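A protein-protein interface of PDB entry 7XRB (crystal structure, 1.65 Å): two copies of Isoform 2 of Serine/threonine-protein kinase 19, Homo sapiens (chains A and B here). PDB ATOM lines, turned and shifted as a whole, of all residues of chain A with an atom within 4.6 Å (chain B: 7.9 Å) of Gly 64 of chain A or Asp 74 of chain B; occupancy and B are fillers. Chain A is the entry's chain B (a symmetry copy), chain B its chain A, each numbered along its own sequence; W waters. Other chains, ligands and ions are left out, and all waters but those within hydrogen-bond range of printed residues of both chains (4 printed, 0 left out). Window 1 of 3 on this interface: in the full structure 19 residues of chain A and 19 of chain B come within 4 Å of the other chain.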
ATOM      1  N   LEU A  60      -1.600  10.226 -13.790  1.00  0.00           N
ATOM      2  CA  LEU A  60      -1.617  11.043 -12.552  1.00  0.00           C
ATOM      3  C   LEU A  60      -1.190  10.178 -11.375  1.00  0.00           C
ATOM      4  O   LEU A  60      -0.513  10.695 -10.481  1.00  0.00           O
ATOM      5  CB  LEU A  60      -3.020  11.602 -12.322  1.00  0.00           C
ATOM      6  CG  LEU A  60      -3.480  12.651 -13.324  1.00  0.00           C
ATOM      7  CD1 LEU A  60      -4.953  12.938 -13.142  1.00  0.00           C
ATOM      8  CD2 LEU A  60      -2.673  13.929 -13.203  1.00  0.00           C
ATOM      9  N   GLN A  61      -1.612   8.913 -11.381  1.00  0.00           N
ATOM     10  CA  GLN A  61      -1.256   7.930 -10.334  1.00  0.00           C
ATOM     11  C   GLN A  61       0.270   7.741 -10.350  1.00  0.00           C
ATOM     12  O   GLN A  61       0.895   7.832  -9.267  1.00  0.00           O
ATOM     13  CB  GLN A  61      -2.042   6.644 -10.580  1.00  0.00           C
ATOM     14  CG  GLN A  61      -1.720   5.554  -9.580  1.00  0.00           C
ATOM     15  CD  GLN A  61      -2.440   4.278  -9.923  1.00  0.00           C
ATOM     16  OE1 GLN A  61      -3.189   4.208 -10.894  1.00  0.00           O
ATOM     17  NE2 GLN A  61      -2.191   3.258  -9.129  1.00  0.00           N
ATOM     18  N   GLU A  62       0.844   7.539 -11.542  1.00  0.00           N
ATOM     19  CA  GLU A  62       2.302   7.325 -11.743  1.00  0.00           C
ATOM     20  C   GLU A  62       3.073   8.589 -11.341  1.00  0.00           C
ATOM     21  O   GLU A  62       4.166   8.432 -10.752  1.00  0.00           O
ATOM     22  CB  GLU A  62       2.579   6.906 -13.189  1.00  0.00           C
ATOM     23  CG  GLU A  62       2.105   5.491 -13.501  1.00  0.00           C
ATOM     24  CD  GLU A  62       2.118   5.102 -14.972  1.00  0.00           C
ATOM     25  OE1 GLU A  62       2.310   6.000 -15.830  1.00  0.00           O
ATOM     26  OE2 GLU A  62       1.941   3.902 -15.257  1.00  0.00           O
ATOM     27  N   GLN A  63       2.514   9.781 -11.592  1.00  0.00           N
ATOM     28  CA  GLN A  63       3.173  11.089 -11.296  1.00  0.00           C
ATOM     29  C   GLN A  63       3.159  11.416  -9.794  1.00  0.00           C
ATOM     30  O   GLN A  63       4.062  12.122  -9.361  1.00  0.00           O
ATOM     31  CB  GLN A  63       2.482  12.223 -12.049  1.00  0.00           C
ATOM     32  CG  GLN A  63       2.768  12.238 -13.537  1.00  0.00           C
ATOM     33  CD  GLN A  63       1.841  13.180 -14.265  1.00  0.00           C
ATOM     34  OE1 GLN A  63       1.387  12.881 -15.365  1.00  0.00           O
ATOM     35  NE2 GLN A  63       1.547  14.318 -13.645  1.00  0.00           N
ATOM     36  N   GLY A  64       2.154  10.954  -9.043  1.00  0.00           N
ATOM     37  CA  GLY A  64       2.128  11.044  -7.569  1.00  0.00           C
ATOM     38  C   GLY A  64       1.545  12.331  -6.992  1.00  0.00           C
ATOM     39  O   GLY A  64       1.568  12.432  -5.764  1.00  0.00           O
ATOM     40  N   GLU A  65       1.036  13.283  -7.782  1.00  0.00           N
ATOM     41  CA  GLU A  65       0.276  14.448  -7.217  1.00  0.00           C
ATOM     42  C   GLU A  65      -1.041  13.947  -6.602  1.00  0.00           C
ATOM     43  O   GLU A  65      -1.489  14.508  -5.583  1.00  0.00           O
ATOM     44  CB  GLU A  65      -0.027  15.531  -8.252  1.00  0.00           C
ATOM     45  CG  GLU A  65      -0.506  16.834  -7.636  1.00  0.00           C
ATOM     46  CD  GLU A  65      -1.066  17.862  -8.605  1.00  0.00           C
ATOM     47  OE1 GLU A  65      -1.388  17.506  -9.766  1.00  0.00           O
ATOM     48  OE2 GLU A  65      -1.198  19.016  -8.192  1.00  0.00           O
ATOM     49  N   ILE A  66      -1.643  12.919  -7.193  1.00  0.00           N
ATOM     50  CA  ILE A  66      -2.816  12.231  -6.584  1.00  0.00           C
ATOM     51  C   ILE A  66      -2.385  10.852  -6.085  1.00  0.00           C
ATOM     52  O   ILE A  66      -1.400  10.284  -6.621  1.00  0.00           O
ATOM     53  CB  ILE A  66      -4.007  12.141  -7.562  1.00  0.00           C
ATOM     54  CG1 ILE A  66      -3.764  11.131  -8.691  1.00  0.00           C
ATOM     55  CG2 ILE A  66      -4.375  13.511  -8.106  1.00  0.00           C
ATOM     56  CD1 ILE A  66      -4.980  10.821  -9.519  1.00  0.00           C
ATOM     57  N   THR A  83      -2.020  13.713  -2.773  1.00  0.00           N
ATOM     58  CA  THR A  83      -0.945  13.151  -1.927  1.00  0.00           C
ATOM     59  C   THR A  83      -0.583  14.145  -0.818  1.00  0.00           C
ATOM     60  O   THR A  83      -0.400  13.690   0.316  1.00  0.00           O
ATOM     61  CB  THR A  83       0.259  12.728  -2.773  1.00  0.00           C
ATOM     62  OG1 THR A  83      -0.232  11.920  -3.846  1.00  0.00           O
ATOM     63  CG2 THR A  83       1.281  11.955  -1.971  1.00  0.00           C
ATOM     64  N   ARG A  87      -0.899  13.306   3.126  1.00  0.00           N
ATOM     65  CA  ARG A  87       0.221  13.550   4.082  1.00  0.00           C
ATOM     66  C   ARG A  87      -0.239  14.485   5.218  1.00  0.00           C
ATOM     67  O   ARG A  87      -0.017  14.144   6.383  1.00  0.00           O
ATOM     68  CB  ARG A  87       1.450  14.117   3.359  1.00  0.00           C
ATOM     69  CG  ARG A  87       2.567  13.112   3.102  1.00  0.00           C
ATOM     70  CD  ARG A  87       3.849  13.821   2.705  1.00  0.00           C
ATOM     71  NE  ARG A  87       3.558  14.570   1.497  1.00  0.00           N
ATOM     72  CZ  ARG A  87       3.855  14.189   0.259  1.00  0.00           C
ATOM     73  NH1 ARG A  87       3.484  14.958  -0.750  1.00  0.00           N
ATOM     74  NH2 ARG A  87       4.520  13.065   0.023  1.00  0.00           N
ATOM     75  N   LEU B  39      13.522  22.516 -11.639  1.00  0.00           N
ATOM     76  CA  LEU B  39      12.349  22.440 -10.748  1.00  0.00           C
ATOM     77  C   LEU B  39      12.590  23.383  -9.587  1.00  0.00           C
ATOM     78  O   LEU B  39      13.751  23.501  -9.157  1.00  0.00           O
ATOM     79  CB  LEU B  39      12.175  21.003 -10.278  1.00  0.00           C
ATOM     80  CG  LEU B  39      11.962  19.970 -11.384  1.00  0.00           C
ATOM     81  CD1 LEU B  39      11.780  18.601 -10.749  1.00  0.00           C
ATOM     82  CD2 LEU B  39      10.757  20.288 -12.246  1.00  0.00           C
ATOM     83  N   SER B  41      11.950  22.797  -6.617  1.00  0.00           N
ATOM     84  CA  SER B  41      12.545  21.948  -5.556  1.00  0.00           C
ATOM     85  C   SER B  41      14.077  22.011  -5.658  1.00  0.00           C
ATOM     86  O   SER B  41      14.740  22.154  -4.630  1.00  0.00           O
ATOM     87  CB  SER B  41      12.059  20.513  -5.640  1.00  0.00           C
ATOM     88  OG  SER B  41      12.278  19.959  -6.936  1.00  0.00           O
ATOM     89  N   LEU B  71       3.681  21.403 -13.484  1.00  0.00           N
ATOM     90  CA  LEU B  71       4.036  20.069 -14.040  1.00  0.00           C
ATOM     91  C   LEU B  71       3.316  18.983 -13.242  1.00  0.00           C
ATOM     92  O   LEU B  71       3.220  17.872 -13.754  1.00  0.00           O
ATOM     93  CB  LEU B  71       5.557  19.886 -14.015  1.00  0.00           C
ATOM     94  CG  LEU B  71       6.338  20.786 -14.972  1.00  0.00           C
ATOM     95  CD1 LEU B  71       7.834  20.577 -14.794  1.00  0.00           C
ATOM     96  CD2 LEU B  71       5.939  20.538 -16.422  1.00  0.00           C
ATOM     97  N   GLY B  72       2.863  19.308 -12.030  1.00  0.00           N
ATOM     98  CA  GLY B  72       2.008  18.443 -11.204  1.00  0.00           C
ATOM     99  C   GLY B  72       2.735  17.271 -10.558  1.00  0.00           C
ATOM    100  O   GLY B  72       2.063  16.260 -10.332  1.00  0.00           O
ATOM    101  N   PHE B  73       4.028  17.371 -10.218  1.00  0.00           N
ATOM    102  CA  PHE B  73       4.701  16.290  -9.439  1.00  0.00           C
ATOM    103  C   PHE B  73       4.259  16.317  -7.984  1.00  0.00           C
ATOM    104  O   PHE B  73       3.869  17.389  -7.491  1.00  0.00           O
ATOM    105  CB  PHE B  73       6.218  16.426  -9.373  1.00  0.00           C
ATOM    106  CG  PHE B  73       6.838  16.356 -10.730  1.00  0.00           C
ATOM    107  CD1 PHE B  73       6.687  15.229 -11.517  1.00  0.00           C
ATOM    108  CD2 PHE B  73       7.519  17.446 -11.243  1.00  0.00           C
ATOM    109  CE1 PHE B  73       7.239  15.183 -12.787  1.00  0.00           C
ATOM    110  CE2 PHE B  73       8.062  17.393 -12.509  1.00  0.00           C
ATOM    111  CZ  PHE B  73       7.915  16.267 -13.281  1.00  0.00           C
ATOM    112  N   ASP B  74       4.414  15.186  -7.296  1.00  0.00           N
ATOM    113  CA  ASP B  74       4.400  15.173  -5.814  1.00  0.00           C
ATOM    114  C   ASP B  74       5.506  16.119  -5.312  1.00  0.00           C
ATOM    115  O   ASP B  74       6.610  16.158  -5.930  1.00  0.00           O
ATOM    116  CB  ASP B  74       4.556  13.751  -5.283  1.00  0.00           C
ATOM    117  CG  ASP B  74       4.217  13.600  -3.814  1.00  0.00           C
ATOM    118  OD1 ASP B  74       3.528  14.502  -3.254  1.00  0.00           O
ATOM    119  OD2 ASP B  74       4.658  12.588  -3.235  1.00  0.00           O
ATOM    120  N   LEU B  75       5.209  16.794  -4.196  1.00  0.00           N
ATOM    121  CA  LEU B  75       6.028  17.865  -3.586  1.00  0.00           C
ATOM    122  C   LEU B  75       6.117  18.973  -4.634  1.00  0.00           C
ATOM    123  O   LEU B  75       5.106  19.147  -5.370  1.00  0.00           O
ATOM    124  CB  LEU B  75       7.388  17.308  -3.145  1.00  0.00           C
ATOM    125  CG  LEU B  75       7.369  16.273  -2.017  1.00  0.00           C
ATOM    126  CD1 LEU B  75       6.475  16.723  -0.875  1.00  0.00           C
ATOM    127  CD2 LEU B  75       6.954  14.902  -2.526  1.00  0.00           C
ATOM    128  N   ASP B  76       7.226  19.704  -4.722  1.00  0.00           N
ATOM    129  CA  ASP B  76       7.226  20.933  -5.557  1.00  0.00           C
ATOM    130  C   ASP B  76       7.053  20.565  -7.033  1.00  0.00           C
ATOM    131  O   ASP B  76       7.994  20.007  -7.659  1.00  0.00           O
ATOM    132  CB  ASP B  76       8.415  21.853  -5.321  1.00  0.00           C
ATOM    133  CG  ASP B  76       7.975  23.287  -5.535  1.00  0.00           C
ATOM    134  OD1 ASP B  76       7.385  23.579  -6.640  1.00  0.00           O
ATOM    135  OD2 ASP B  76       8.148  24.080  -4.584  1.00  0.00           O
ATOM    136  N   ALA B  77       5.869  20.903  -7.548  1.00  0.00           N
ATOM    137  CA  ALA B  77       5.378  20.598  -8.903  1.00  0.00           C
ATOM    138  C   ALA B  77       5.553  21.789  -9.848  1.00  0.00           C
ATOM    139  O   ALA B  77       4.749  21.827 -10.793  1.00  0.00           O
ATOM    140  CB  ALA B  77       3.915  20.265  -8.802  1.00  0.00           C
ATOM    141  N   HIS B  78       6.488  22.719  -9.609  1.00  0.00           N
ATOM    142  CA  HIS B  78       6.722  23.851 -10.547  1.00  0.00           C
ATOM    143  C   HIS B  78       8.017  23.665 -11.331  1.00  0.00           C
ATOM    144  O   HIS B  78       9.084  23.582 -10.698  1.00  0.00           O
ATOM    145  CB  HIS B  78       6.761  25.202  -9.844  1.00  0.00           C
ATOM    146  CG  HIS B  78       5.441  25.688  -9.369  1.00  0.00           C
ATOM    147  ND1 HIS B  78       5.327  26.770  -8.517  1.00  0.00           N
ATOM    148  CD2 HIS B  78       4.190  25.221  -9.579  1.00  0.00           C
ATOM    149  CE1 HIS B  78       4.056  26.955  -8.218  1.00  0.00           C
ATOM    150  NE2 HIS B  78       3.335  26.013  -8.855  1.00  0.00           N
ATOM    151  N   ILE B 163       8.257  14.394 -17.916  1.00  0.00           N
ATOM    152  CA  ILE B 163       7.538  14.015 -16.666  1.00  0.00           C
ATOM    153  C   ILE B 163       7.719  12.506 -16.445  1.00  0.00           C
ATOM    154  O   ILE B 163       8.010  12.097 -15.296  1.00  0.00           O
ATOM    155  CB  ILE B 163       6.059  14.438 -16.734  1.00  0.00           C
ATOM    156  CG1 ILE B 163       5.933  15.963 -16.701  1.00  0.00           C
ATOM    157  CG2 ILE B 163       5.251  13.773 -15.622  1.00  0.00           C
ATOM    158  CD1 ILE B 163       4.586  16.496 -17.121  1.00  0.00           C
ATOM    159  N   PHE B 166      11.304  11.798 -15.441  1.00  0.00           N
ATOM    160  CA  PHE B 166      11.584  12.424 -14.135  1.00  0.00           C
ATOM    161  C   PHE B 166      11.013  11.553 -13.013  1.00  0.00           C
ATOM    162  O   PHE B 166      11.723  11.274 -12.040  1.00  0.00           O
ATOM    163  CB  PHE B 166      11.052  13.843 -14.043  1.00  0.00           C
ATOM    164  CG  PHE B 166      11.302  14.399 -12.675  1.00  0.00           C
ATOM    165  CD1 PHE B 166      12.555  14.858 -12.322  1.00  0.00           C
ATOM    166  CD2 PHE B 166      10.307  14.370 -11.719  1.00  0.00           C
ATOM    167  CE1 PHE B 166      12.793  15.325 -11.043  1.00  0.00           C
ATOM    168  CE2 PHE B 166      10.544  14.840 -10.442  1.00  0.00           C
ATOM    169  CZ  PHE B 166      11.779  15.335 -10.118  1.00  0.00           C
ATOM    170  N   VAL B 167       9.759  11.135 -13.129  1.00  0.00           N
ATOM    171  CA  VAL B 167       9.116  10.351 -12.040  1.00  0.00           C
ATOM    172  C   VAL B 167       9.863   9.028 -11.856  1.00  0.00           C
ATOM    173  O   VAL B 167      10.168   8.675 -10.697  1.00  0.00           O
ATOM    174  CB  VAL B 167       7.620  10.157 -12.336  1.00  0.00           C
ATOM    175  CG1 VAL B 167       7.001   9.106 -11.432  1.00  0.00           C
ATOM    176  CG2 VAL B 167       6.878  11.478 -12.230  1.00  0.00           C
ATOM    177  N   ARG B 170      13.325   9.753 -10.229  1.00  0.00           N
ATOM    178  CA  ARG B 170      13.188  10.160  -8.813  1.00  0.00           C
ATOM    179  C   ARG B 170      13.028   8.895  -7.958  1.00  0.00           C
ATOM    180  O   ARG B 170      13.717   8.757  -6.947  1.00  0.00           O
ATOM    181  CB  ARG B 170      12.010  11.120  -8.670  1.00  0.00           C
ATOM    182  CG  ARG B 170      11.670  11.482  -7.239  1.00  0.00           C
ATOM    183  CD  ARG B 170      10.301  12.148  -7.211  1.00  0.00           C
ATOM    184  NE  ARG B 170      10.447  13.567  -7.013  1.00  0.00           N
ATOM    185  CZ  ARG B 170       9.456  14.401  -6.765  1.00  0.00           C
ATOM    186  NH1 ARG B 170       9.721  15.676  -6.564  1.00  0.00           N
ATOM    187  NH2 ARG B 170       8.203  13.969  -6.702  1.00  0.00           N
ATOM    188  N   GLN B 171      12.162   7.982  -8.372  1.00  0.00           N
ATOM    189  CA  GLN B 171      11.921   6.740  -7.593  1.00  0.00           C
ATOM    190  C   GLN B 171      13.208   5.897  -7.548  1.00  0.00           C
ATOM    191  O   GLN B 171      13.567   5.363  -6.481  1.00  0.00           O
ATOM    192  CB  GLN B 171      10.774   5.967  -8.226  1.00  0.00           C
ATOM    193  CG  GLN B 171       9.430   6.649  -8.064  1.00  0.00           C
ATOM    194  CD  GLN B 171       8.360   6.053  -8.951  1.00  0.00           C
ATOM    195  OE1 GLN B 171       8.587   5.112  -9.714  1.00  0.00           O
ATOM    196  NE2 GLN B 171       7.163   6.596  -8.845  1.00  0.00           N
ATOM    197  N   ASP B 209      16.622  17.605  -6.553  1.00  0.00           N
ATOM    198  CA  ASP B 209      15.150  17.520  -6.389  1.00  0.00           C
ATOM    199  C   ASP B 209      14.842  16.822  -5.059  1.00  0.00           C
ATOM    200  O   ASP B 209      13.991  17.338  -4.303  1.00  0.00           O
ATOM    201  CB  ASP B 209      14.473  16.832  -7.568  1.00  0.00           C
ATOM    202  CG  ASP B 209      13.056  16.413  -7.209  1.00  0.00           C
ATOM    203  OD1 ASP B 209      12.178  17.308  -7.090  1.00  0.00           O
ATOM    204  OD2 ASP B 209      12.855  15.183  -7.026  1.00  0.00           O
ATOM    205  N   ALA B 213      12.849  18.896  -2.226  1.00  0.00           N
ATOM    206  CA  ALA B 213      11.488  18.371  -1.952  1.00  0.00           C
ATOM    207  C   ALA B 213      11.431  17.716  -0.564  1.00  0.00           C
ATOM    208  O   ALA B 213      10.318  17.291  -0.148  1.00  0.00           O
ATOM    209  CB  ALA B 213      11.088  17.394  -3.030  1.00  0.00           C
ATOM    210  N   LEU B 215      12.503  14.883   0.287  1.00  0.00           N
ATOM    211  CA  LEU B 215      12.370  13.407   0.167  1.00  0.00           C
ATOM    212  C   LEU B 215      13.577  12.711   0.797  1.00  0.00           C
ATOM    213  O   LEU B 215      13.450  11.542   1.178  1.00  0.00           O
ATOM    214  CB  LEU B 215      12.213  13.047  -1.308  1.00  0.00           C
ATOM    215  CG  LEU B 215      10.851  13.427  -1.884  1.00  0.00           C
ATOM    216  CD1 LEU B 215      10.848  13.324  -3.405  1.00  0.00           C
ATOM    217  CD2 LEU B 215       9.779  12.531  -1.270  1.00  0.00           C
HETATM  218  O   HOH W   1       1.314  16.759 -15.263  1.00  0.00           O
HETATM  219  O   HOH W   2       6.442  11.926  -8.280  1.00  0.00           O
HETATM  220  O   HOH W   3       5.451   6.006 -10.950  1.00  0.00           O
HETATM  221  O   HOH W   4      -0.382  15.553 -11.304  1.00  0.00           O
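Of the printed residues of chain B, Gln 63 of chain A touches Leu 71, Gly 72, Asp 74, Ile 163 and Val 167. Gly 64 of chain A touches just one residue of chain B: Asp 74 (3.3 Å). Leu 39 of chain B touches none of the printed residues of chain A. Printed residues of chain A within 4 Å of Leu 71 of chain B: Gln 63. Of the printed residues of chain A, Gly 72 of chain B touches Gln 63 and Glu 65. Phe 73 of chain B touches none of the printed residues of chain A. Printed residues of chain A within 4 Å of Asp 74 of chain B: Gln 63 (3.7 Å), Gly 64 (3.3 Å), Glu 65 (3.9 Å), Thr 83 (3.6 Å) and Arg 87 (2.5 Å). Printed residues of chain A within 4 Å of Leu 75 of chain B: Arg 87. Of the printed residues of chain A, Gln 171 of chain B touches Glu 62 (3.999 Å). The nearest printed residue of chain A that does not touch Asp 74 of chain B is Ile 66 of chain A (6.5 Å).
The guanidinium group (NH1) of Arg 87 of chain A is in salt-bridge range of the side-chain carboxylate (OD1) of Asp 74 of chain B (2.5 Å).
The backbone carbonyl oxygen (O) of Ala 77 of chain B lies within hydrogen-bond range of the backbone NH (N) of Leu 71 of chain B. O of Ala 77 of chain B sits at hydrogen-bond distance from N of Gly 72 of chain B (3.4 Å). O of Asp 74 of chain B lies within hydrogen-bond range of NH2 of Arg 170 of chain B. The side-chain hydroxyl (OG1) of Thr 83 of chain A lies within hydrogen-bond range of the backbone carbonyl oxygen (O) of Gly 64 of chain A (2.7 Å). The backbone NH of Thr 83 of chain A lies within hydrogen-bond range of the backbone carbonyl oxygen of Glu 65 of chain A, 3.0 Å away. O of Ile 66 of chain A sits close to OG1 of Thr 83 of chain A, 3.4 Å away.
No position is printed for both chains. Of the 13 pairs that touch across the chains among the printed residues, none has its exchanged pair printed and touching as well.
Water W2 lies within hydrogen-bond range of the backbone carbonyl oxygen (O) of Gln 63 of chain A (2.6 Å) and the guanidinium group (NH2) of Arg 170 of chain B (3.1 Å). Water W1 lies within hydrogen-bond range of the backbone carbonyl oxygen of Leu 71 of chain B and the side-chain amide nitrogen of Gln 63 of chain A. Water W4 lies within hydrogen-bond range of OE1 of Glu 65 of chain A, O of Gly 72 of chain B and NE2 of Gln 63 of chain A. Water W3 lies within hydrogen-bond range of the backbone carbonyl oxygen of Glu 62 of chain A and the side-chain amide nitrogen of Gln 171 of chain B.
Gln 63 of chain A touches Leu 71 of chain B. Gly 72 of chain B touches Gln 63 of chain A (O to NE2, 3.9 Å). Gln 63 of chain A touches Asp 74 of chain B. Ile 163 of chain B touches Gln 63 of chain A. CA of Gln 63 of chain A touches CG2 of Val 167 of chain B, 3.8 Å away. Gly 64 of chain A touches Asp 74 of chain B (O to CB, 3.3 Å). Glu 65 of chain A touches Gly 72 of chain B. Glu 65 of chain A touches Asp 74 of chain B. Thr 83 of chain A touches Asp 74 of chain B (CG2 to OD1, 3.6 Å). Arg 87 of chain A touches Leu 75 of chain B.
Of the 18 printed residues of chain B, 7 touch a printed residue of chain A. Of the 9 printed residues of chain A, 6 touch a printed residue of chain B. Among the printed residues, 13 pairs touch across the chains.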
